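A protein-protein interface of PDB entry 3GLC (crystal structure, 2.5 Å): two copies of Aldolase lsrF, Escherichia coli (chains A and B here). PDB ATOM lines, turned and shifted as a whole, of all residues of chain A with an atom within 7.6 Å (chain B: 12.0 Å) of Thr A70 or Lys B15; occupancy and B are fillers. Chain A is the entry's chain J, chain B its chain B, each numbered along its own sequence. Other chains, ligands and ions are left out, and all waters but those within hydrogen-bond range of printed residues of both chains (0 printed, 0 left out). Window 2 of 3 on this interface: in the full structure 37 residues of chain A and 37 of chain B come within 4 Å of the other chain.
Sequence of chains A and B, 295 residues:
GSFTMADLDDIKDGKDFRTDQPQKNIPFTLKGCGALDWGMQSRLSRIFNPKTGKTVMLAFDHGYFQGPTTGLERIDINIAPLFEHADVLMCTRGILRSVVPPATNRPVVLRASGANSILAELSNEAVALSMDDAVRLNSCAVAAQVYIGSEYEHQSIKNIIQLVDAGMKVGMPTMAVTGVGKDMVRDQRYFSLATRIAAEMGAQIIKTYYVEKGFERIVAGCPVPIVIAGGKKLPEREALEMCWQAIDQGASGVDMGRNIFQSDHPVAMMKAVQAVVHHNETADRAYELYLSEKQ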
ATOM      1  N   HIS A  62      15.787  33.512  26.673  1.00  0.00           N
ATOM      2  CA  HIS A  62      14.642  33.939  25.871  1.00  0.00           C
ATOM      3  C   HIS A  62      13.311  33.765  26.610  1.00  0.00           C
ATOM      4  O   HIS A  62      12.342  34.473  26.334  1.00  0.00           O
ATOM      5  CB  HIS A  62      14.609  33.172  24.549  1.00  0.00           C
ATOM      6  CG  HIS A  62      15.941  33.090  23.871  1.00  0.00           C
ATOM      7  ND1 HIS A  62      16.168  33.573  22.601  1.00  0.00           N
ATOM      8  CD2 HIS A  62      17.125  32.599  24.302  1.00  0.00           C
ATOM      9  CE1 HIS A  62      17.436  33.389  22.282  1.00  0.00           C
ATOM     10  NE2 HIS A  62      18.040  32.801  23.297  1.00  0.00           N
ATOM     11  N   GLN A  66       9.161  35.395  26.799  1.00  0.00           N
ATOM     12  CA  GLN A  66       8.541  34.598  25.725  1.00  0.00           C
ATOM     13  C   GLN A  66       7.941  33.278  26.166  1.00  0.00           C
ATOM     14  O   GLN A  66       7.207  32.653  25.399  1.00  0.00           O
ATOM     15  CB  GLN A  66       9.533  34.295  24.616  1.00  0.00           C
ATOM     16  CG  GLN A  66       9.961  35.498  23.859  1.00  0.00           C
ATOM     17  CD  GLN A  66      11.023  35.205  22.833  1.00  0.00           C
ATOM     18  OE1 GLN A  66      10.900  34.268  22.041  1.00  0.00           O
ATOM     19  NE2 GLN A  66      12.079  36.023  22.823  1.00  0.00           N
ATOM     20  N   GLY A  67       8.221  32.840  27.392  1.00  0.00           N
ATOM     21  CA  GLY A  67       7.741  31.530  27.808  1.00  0.00           C
ATOM     22  C   GLY A  67       8.548  30.464  27.086  1.00  0.00           C
ATOM     23  O   GLY A  67       9.632  30.766  26.562  1.00  0.00           O
ATOM     24  N   PRO A  68       8.018  29.217  27.049  1.00  0.00           N
ATOM     25  CA  PRO A  68       8.770  28.094  26.500  1.00  0.00           C
ATOM     26  C   PRO A  68       8.887  28.230  24.993  1.00  0.00           C
ATOM     27  O   PRO A  68       8.009  27.811  24.270  1.00  0.00           O
ATOM     28  CB  PRO A  68       7.911  26.871  26.871  1.00  0.00           C
ATOM     29  CG  PRO A  68       6.677  27.417  27.554  1.00  0.00           C
ATOM     30  CD  PRO A  68       6.609  28.857  27.300  1.00  0.00           C
ATOM     31  N   THR A  69       9.971  28.832  24.546  1.00  0.00           N
ATOM     32  CA  THR A  69      10.202  29.088  23.147  1.00  0.00           C
ATOM     33  C   THR A  69      10.859  27.834  22.495  1.00  0.00           C
ATOM     34  O   THR A  69      11.440  27.002  23.214  1.00  0.00           O
ATOM     35  CB  THR A  69      11.059  30.370  23.022  1.00  0.00           C
ATOM     36  OG1 THR A  69      11.163  30.773  21.656  1.00  0.00           O
ATOM     37  CG2 THR A  69      12.449  30.135  23.569  1.00  0.00           C
ATOM     38  N   THR A  70      10.760  27.694  21.165  1.00  0.00           N
ATOM     39  CA  THR A  70      11.239  26.480  20.448  1.00  0.00           C
ATOM     40  C   THR A  70      12.714  26.162  20.649  1.00  0.00           C
ATOM     41  O   THR A  70      13.575  26.945  20.284  1.00  0.00           O
ATOM     42  CB  THR A  70      11.002  26.585  18.929  1.00  0.00           C
ATOM     43  OG1 THR A  70       9.601  26.784  18.685  1.00  0.00           O
ATOM     44  CG2 THR A  70      11.491  25.295  18.209  1.00  0.00           C
ATOM     45  N   GLY A  71      12.991  24.985  21.202  1.00  0.00           N
ATOM     46  CA  GLY A  71      14.362  24.587  21.520  1.00  0.00           C
ATOM     47  C   GLY A  71      14.659  24.721  23.014  1.00  0.00           C
ATOM     48  O   GLY A  71      15.564  24.062  23.538  1.00  0.00           O
ATOM     49  N   LEU A  72      13.893  25.570  23.701  1.00  0.00           N
ATOM     50  CA  LEU A  72      14.123  25.831  25.105  1.00  0.00           C
ATOM     51  C   LEU A  72      13.002  25.283  25.955  1.00  0.00           C
ATOM     52  O   LEU A  72      12.841  25.667  27.122  1.00  0.00           O
ATOM     53  CB  LEU A  72      14.314  27.337  25.368  1.00  0.00           C
ATOM     54  CG  LEU A  72      15.485  27.963  24.628  1.00  0.00           C
ATOM     55  CD1 LEU A  72      15.591  29.454  24.902  1.00  0.00           C
ATOM     56  CD2 LEU A  72      16.788  27.267  24.969  1.00  0.00           C
ATOM     57  N   GLU A  73      12.208  24.389  25.389  1.00  0.00           N
ATOM     58  CA  GLU A  73      11.123  23.812  26.159  1.00  0.00           C
ATOM     59  C   GLU A  73      11.710  23.070  27.363  1.00  0.00           C
ATOM     60  O   GLU A  73      11.132  23.099  28.456  1.00  0.00           O
ATOM     61  CB  GLU A  73      10.255  22.878  25.308  1.00  0.00           C
ATOM     62  CG  GLU A  73       9.718  23.501  24.020  1.00  0.00           C
ATOM     63  CD  GLU A  73      10.650  23.313  22.796  1.00  0.00           C
ATOM     64  OE1 GLU A  73      11.881  23.085  22.955  1.00  0.00           O
ATOM     65  OE2 GLU A  73      10.128  23.389  21.662  1.00  0.00           O
ATOM     66  N   ARG A  74      12.853  22.402  27.154  1.00  0.00           N
ATOM     67  CA  ARG A  74      13.460  21.574  28.189  1.00  0.00           C
ATOM     68  C   ARG A  74      14.939  21.873  28.259  1.00  0.00           C
ATOM     69  O   ARG A  74      15.738  21.194  27.644  1.00  0.00           O
ATOM     70  CB  ARG A  74      13.228  20.087  27.915  1.00  0.00           C
ATOM     71  CG  ARG A  74      11.753  19.653  27.948  1.00  0.00           C
ATOM     72  CD  ARG A  74      11.169  19.721  29.346  1.00  0.00           C
ATOM     73  NE  ARG A  74      11.937  18.903  30.284  1.00  0.00           N
ATOM     74  CZ  ARG A  74      11.636  17.643  30.600  1.00  0.00           C
ATOM     75  NH1 ARG A  74      10.567  17.049  30.064  1.00  0.00           N
ATOM     76  NH2 ARG A  74      12.394  16.969  31.463  1.00  0.00           N
ATOM     77  N   ASN A  78      17.798  19.297  26.771  1.00  0.00           N
ATOM     78  CA  ASN A  78      18.225  19.721  25.456  1.00  0.00           C
ATOM     79  C   ASN A  78      19.491  20.567  25.497  1.00  0.00           C
ATOM     80  O   ASN A  78      20.405  20.366  24.699  1.00  0.00           O
ATOM     81  CB  ASN A  78      17.083  20.545  24.865  1.00  0.00           C
ATOM     82  CG  ASN A  78      16.923  20.348  23.403  1.00  0.00           C
ATOM     83  OD1 ASN A  78      16.631  19.236  22.945  1.00  0.00           O
ATOM     84  ND2 ASN A  78      17.088  21.442  22.635  1.00  0.00           N
ATOM     85  N   ILE A  79      19.536  21.515  26.440  1.00  0.00           N
ATOM     86  CA  ILE A  79      20.604  22.526  26.515  1.00  0.00           C
ATOM     87  C   ILE A  79      21.754  22.121  27.438  1.00  0.00           C
ATOM     88  O   ILE A  79      22.920  22.496  27.192  1.00  0.00           O
ATOM     89  CB  ILE A  79      20.050  23.901  26.968  1.00  0.00           C
ATOM     90  CG1 ILE A  79      18.869  24.306  26.091  1.00  0.00           C
ATOM     91  CG2 ILE A  79      21.131  24.961  26.904  1.00  0.00           C
ATOM     92  CD1 ILE A  79      19.221  24.388  24.618  1.00  0.00           C
ATOM     93  N   ILE A 118       5.564  39.081  25.382  1.00  0.00           N
ATOM     94  CA  ILE A 118       5.153  39.127  24.001  1.00  0.00           C
ATOM     95  C   ILE A 118       3.698  39.554  23.873  1.00  0.00           C
ATOM     96  O   ILE A 118       3.256  39.918  22.787  1.00  0.00           O
ATOM     97  CB  ILE A 118       5.322  37.761  23.322  1.00  0.00           C
ATOM     98  CG1 ILE A 118       4.596  36.660  24.127  1.00  0.00           C
ATOM     99  CG2 ILE A 118       6.790  37.432  23.168  1.00  0.00           C
ATOM    100  CD1 ILE A 118       4.542  35.301  23.442  1.00  0.00           C
ATOM    101  N   ARG A 258      19.574  30.628  19.137  1.00  0.00           N
ATOM    102  CA  ARG A 258      18.791  29.853  18.186  1.00  0.00           C
ATOM    103  C   ARG A 258      19.703  29.133  17.198  1.00  0.00           C
ATOM    104  O   ARG A 258      19.558  27.929  16.989  1.00  0.00           O
ATOM    105  CB  ARG A 258      17.778  30.736  17.448  1.00  0.00           C
ATOM    106  CG  ARG A 258      16.722  31.405  18.320  1.00  0.00           C
ATOM    107  CD  ARG A 258      15.679  32.064  17.435  1.00  0.00           C
ATOM    108  NE  ARG A 258      15.089  33.269  18.035  1.00  0.00           N
ATOM    109  CZ  ARG A 258      15.569  34.510  17.921  1.00  0.00           C
ATOM    110  NH1 ARG A 258      16.668  34.764  17.241  1.00  0.00           N
ATOM    111  NH2 ARG A 258      14.951  35.515  18.503  1.00  0.00           N
ATOM    112  N   PHE A 261      21.060  26.100  19.523  1.00  0.00           N
ATOM    113  CA  PHE A 261      20.129  25.156  20.112  1.00  0.00           C
ATOM    114  C   PHE A 261      19.014  24.709  19.190  1.00  0.00           C
ATOM    115  O   PHE A 261      18.344  23.732  19.489  1.00  0.00           O
ATOM    116  CB  PHE A 261      19.606  25.580  21.491  1.00  0.00           C
ATOM    117  CG  PHE A 261      18.841  26.865  21.522  1.00  0.00           C
ATOM    118  CD1 PHE A 261      17.539  26.928  21.066  1.00  0.00           C
ATOM    119  CD2 PHE A 261      19.399  27.992  22.105  1.00  0.00           C
ATOM    120  CE1 PHE A 261      16.817  28.117  21.120  1.00  0.00           C
ATOM    121  CE2 PHE A 261      18.680  29.194  22.179  1.00  0.00           C
ATOM    122  CZ  PHE A 261      17.386  29.254  21.685  1.00  0.00           C
ATOM    123  N   GLN A 262      18.829  25.398  18.067  1.00  0.00           N
ATOM    124  CA  GLN A 262      17.844  24.962  17.071  1.00  0.00           C
ATOM    125  C   GLN A 262      18.456  24.187  15.907  1.00  0.00           C
ATOM    126  O   GLN A 262      17.732  23.735  15.025  1.00  0.00           O
ATOM    127  CB  GLN A 262      17.031  26.144  16.559  1.00  0.00           C
ATOM    128  CG  GLN A 262      15.873  26.536  17.475  1.00  0.00           C
ATOM    129  CD  GLN A 262      15.069  27.727  16.950  1.00  0.00           C
ATOM    130  OE1 GLN A 262      15.365  28.293  15.872  1.00  0.00           O
ATOM    131  NE2 GLN A 262      14.039  28.115  17.710  1.00  0.00           N
ATOM    132  N   GLY B  14       4.949  22.676  16.313  1.00  0.00           N
ATOM    133  CA  GLY B  14       6.323  22.115  16.121  1.00  0.00           C
ATOM    134  C   GLY B  14       7.256  22.270  17.323  1.00  0.00           C
ATOM    135  O   GLY B  14       8.458  22.548  17.153  1.00  0.00           O
ATOM    136  N   LYS B  15       6.708  22.091  18.534  1.00  0.00           N
ATOM    137  CA  LYS B  15       7.486  22.161  19.791  1.00  0.00           C
ATOM    138  C   LYS B  15       7.560  20.786  20.489  1.00  0.00           C
ATOM    139  O   LYS B  15       6.579  20.012  20.477  1.00  0.00           O
ATOM    140  CB  LYS B  15       6.907  23.236  20.743  1.00  0.00           C
ATOM    141  CG  LYS B  15       7.087  24.671  20.232  1.00  0.00           C
ATOM    142  CD  LYS B  15       6.681  25.753  21.236  1.00  0.00           C
ATOM    143  CE  LYS B  15       6.969  27.111  20.608  1.00  0.00           C
ATOM    144  NZ  LYS B  15       6.401  28.251  21.369  1.00  0.00           N
ATOM    145  N   ASP B  16       8.717  20.489  21.093  1.00  0.00           N
ATOM    146  CA  ASP B  16       8.895  19.213  21.810  1.00  0.00           C
ATOM    147  C   ASP B  16       9.251  19.312  23.320  1.00  0.00           C
ATOM    148  O   ASP B  16      10.399  19.526  23.702  1.00  0.00           O
ATOM    149  CB  ASP B  16       9.882  18.311  21.054  1.00  0.00           C
ATOM    150  CG  ASP B  16       9.928  16.902  21.614  1.00  0.00           C
ATOM    151  OD1 ASP B  16       8.881  16.403  22.131  1.00  0.00           O
ATOM    152  OD2 ASP B  16      11.031  16.310  21.540  1.00  0.00           O
ATOM    153  N   PHE B  17       8.243  19.095  24.156  1.00  0.00           N
ATOM    154  CA  PHE B  17       8.370  19.209  25.590  1.00  0.00           C
ATOM    155  C   PHE B  17       8.838  17.935  26.256  1.00  0.00           C
ATOM    156  O   PHE B  17       9.092  17.940  27.467  1.00  0.00           O
ATOM    157  CB  PHE B  17       7.020  19.599  26.183  1.00  0.00           C
ATOM    158  CG  PHE B  17       6.598  20.993  25.846  1.00  0.00           C
ATOM    159  CD1 PHE B  17       6.837  22.033  26.735  1.00  0.00           C
ATOM    160  CD2 PHE B  17       5.957  21.269  24.641  1.00  0.00           C
ATOM    161  CE1 PHE B  17       6.456  23.336  26.437  1.00  0.00           C
ATOM    162  CE2 PHE B  17       5.577  22.566  24.323  1.00  0.00           C
ATOM    163  CZ  PHE B  17       5.832  23.613  25.232  1.00  0.00           C
ATOM    164  N   ARG B  18       8.906  16.839  25.496  1.00  0.00           N
ATOM    165  CA  ARG B  18       9.451  15.580  25.980  1.00  0.00           C
ATOM    166  C   ARG B  18       8.762  15.144  27.264  1.00  0.00           C
ATOM    167  O   ARG B  18       9.417  14.806  28.243  1.00  0.00           O
ATOM    168  CB  ARG B  18      10.959  15.713  26.192  1.00  0.00           C
ATOM    169  CG  ARG B  18      11.693  16.365  25.018  1.00  0.00           C
ATOM    170  CD  ARG B  18      12.868  15.516  24.596  1.00  0.00           C
ATOM    171  NE  ARG B  18      12.563  14.129  24.948  1.00  0.00           N
ATOM    172  CZ  ARG B  18      13.462  13.183  25.189  1.00  0.00           C
ATOM    173  NH1 ARG B  18      14.765  13.440  25.090  1.00  0.00           N
ATOM    174  NH2 ARG B  18      13.042  11.974  25.535  1.00  0.00           N
ATOM    175  N   THR B  19       7.431  15.147  27.237  1.00  0.00           N
ATOM    176  CA  THR B  19       6.595  14.891  28.414  1.00  0.00           C
ATOM    177  C   THR B  19       6.697  13.462  28.932  1.00  0.00           C
ATOM    178  O   THR B  19       6.142  13.134  29.987  1.00  0.00           O
ATOM    179  CB  THR B  19       5.105  15.140  28.098  1.00  0.00           C
ATOM    180  OG1 THR B  19       4.691  14.268  27.037  1.00  0.00           O
ATOM    181  CG2 THR B  19       4.872  16.558  27.654  1.00  0.00           C
ATOM    182  N   ASP B  20       7.358  12.606  28.160  1.00  0.00           N
ATOM    183  CA  ASP B  20       7.592  11.214  28.535  1.00  0.00           C
ATOM    184  C   ASP B  20       8.867  11.052  29.407  1.00  0.00           C
ATOM    185  O   ASP B  20       9.143   9.968  29.921  1.00  0.00           O
ATOM    186  CB  ASP B  20       7.664  10.333  27.275  1.00  0.00           C
ATOM    187  CG  ASP B  20       8.834  10.696  26.340  1.00  0.00           C
ATOM    188  OD1 ASP B  20       9.387  11.822  26.386  1.00  0.00           O
ATOM    189  OD2 ASP B  20       9.192   9.828  25.517  1.00  0.00           O
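O of Phe B17 sits at hydrogen-bond distance from NH1 of Arg A74.
The backbone carbonyl oxygen (O) of Arg B18 sits at hydrogen-bond distance from the guanidinium group (NH1) of Arg A74 (3.1 Å).
The side-chain carboxylate of Glu A73 sits at hydrogen-bond distance from the backbone NH of Asp B16.
The backbone carbonyl oxygen of Pro A68 sits at hydrogen-bond distance from the side-chain amino group of Lys B15, 3.3 Å away.
OD1 of Asp B16 lies close to N of Arg B18.
The backbone NH of Gly A71 sits at hydrogen-bond distance from the side-chain carboxylate of Glu A73 (2.8 Å).
The backbone carbonyl oxygen (O) of Thr A70 is in hydrogen-bond range of the side-chain amide nitrogen (NE2) of Gln A262 (2.9 Å).
The side-chain carboxylate (OD1) of Asp B20 is in salt-bridge range of the guanidinium group (NH2) of Arg B18, at 3.8 Å.
Phe B17 touches Pro A68 (CE1 to CB, 3.8 Å).
Thr A70 touches Lys B15.
Glu A73 touches Lys B15.
Glu A73 touches Phe B17.
His A62 touches none of the printed residues of chain B.
No residue of chain B comes within 4 Å of Gly A67.
Pro A68 touches just these residues of chain B: Lys B15 and Phe B17.
No residue of chain B comes within 4 Å of Thr A69.
Thr A70 touches one residue of chain B.
Gly A71 touches none of the printed residues of chain B.
No residue of chain B comes within 4 Å of Leu A72.
Printed residues of chain B within 4 Å of Glu A73: Lys B15, Asp B16 and Phe B17.
Of the printed residues of chain B, Arg A74 touches Phe B17 (3.1 Å) and Arg B18 (3.1 Å).
Ile A79 touches none of the printed residues of chain B.
No residue of chain B comes within 4 Å of Phe A261.
No residue of chain B comes within 4 Å of Gln A262.
Lys B15 touches just these residues of chain A: Pro A68, Thr A70 and Glu A73.
Printed residues of chain A within 4 Å of Asp B16: Glu A73 (3.3 Å).
Printed residues of chain A within 4 Å of Phe B17: Pro A68 (3.8 Å), Glu A73 (3.8 Å) and Arg A74 (3.1 Å).
Printed residues of chain A within 4 Å of Arg B18: Arg A74.
The nearest residue of chain B that does not touch Thr A70 is Gly B14 (4.2 Å).
Printed residues of chain A that touch a printed residue of chain B: Pro A68, Thr A70, Glu A73 and Arg A74.
Printed residues of chain B that touch a printed residue of chain A: Lys B15, Asp B16, Phe B17 and Arg B18.
Hydrophobic or aromatic side chains of chain B that line the printed part of chain A: Phe B17.
No position is printed for both chains.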
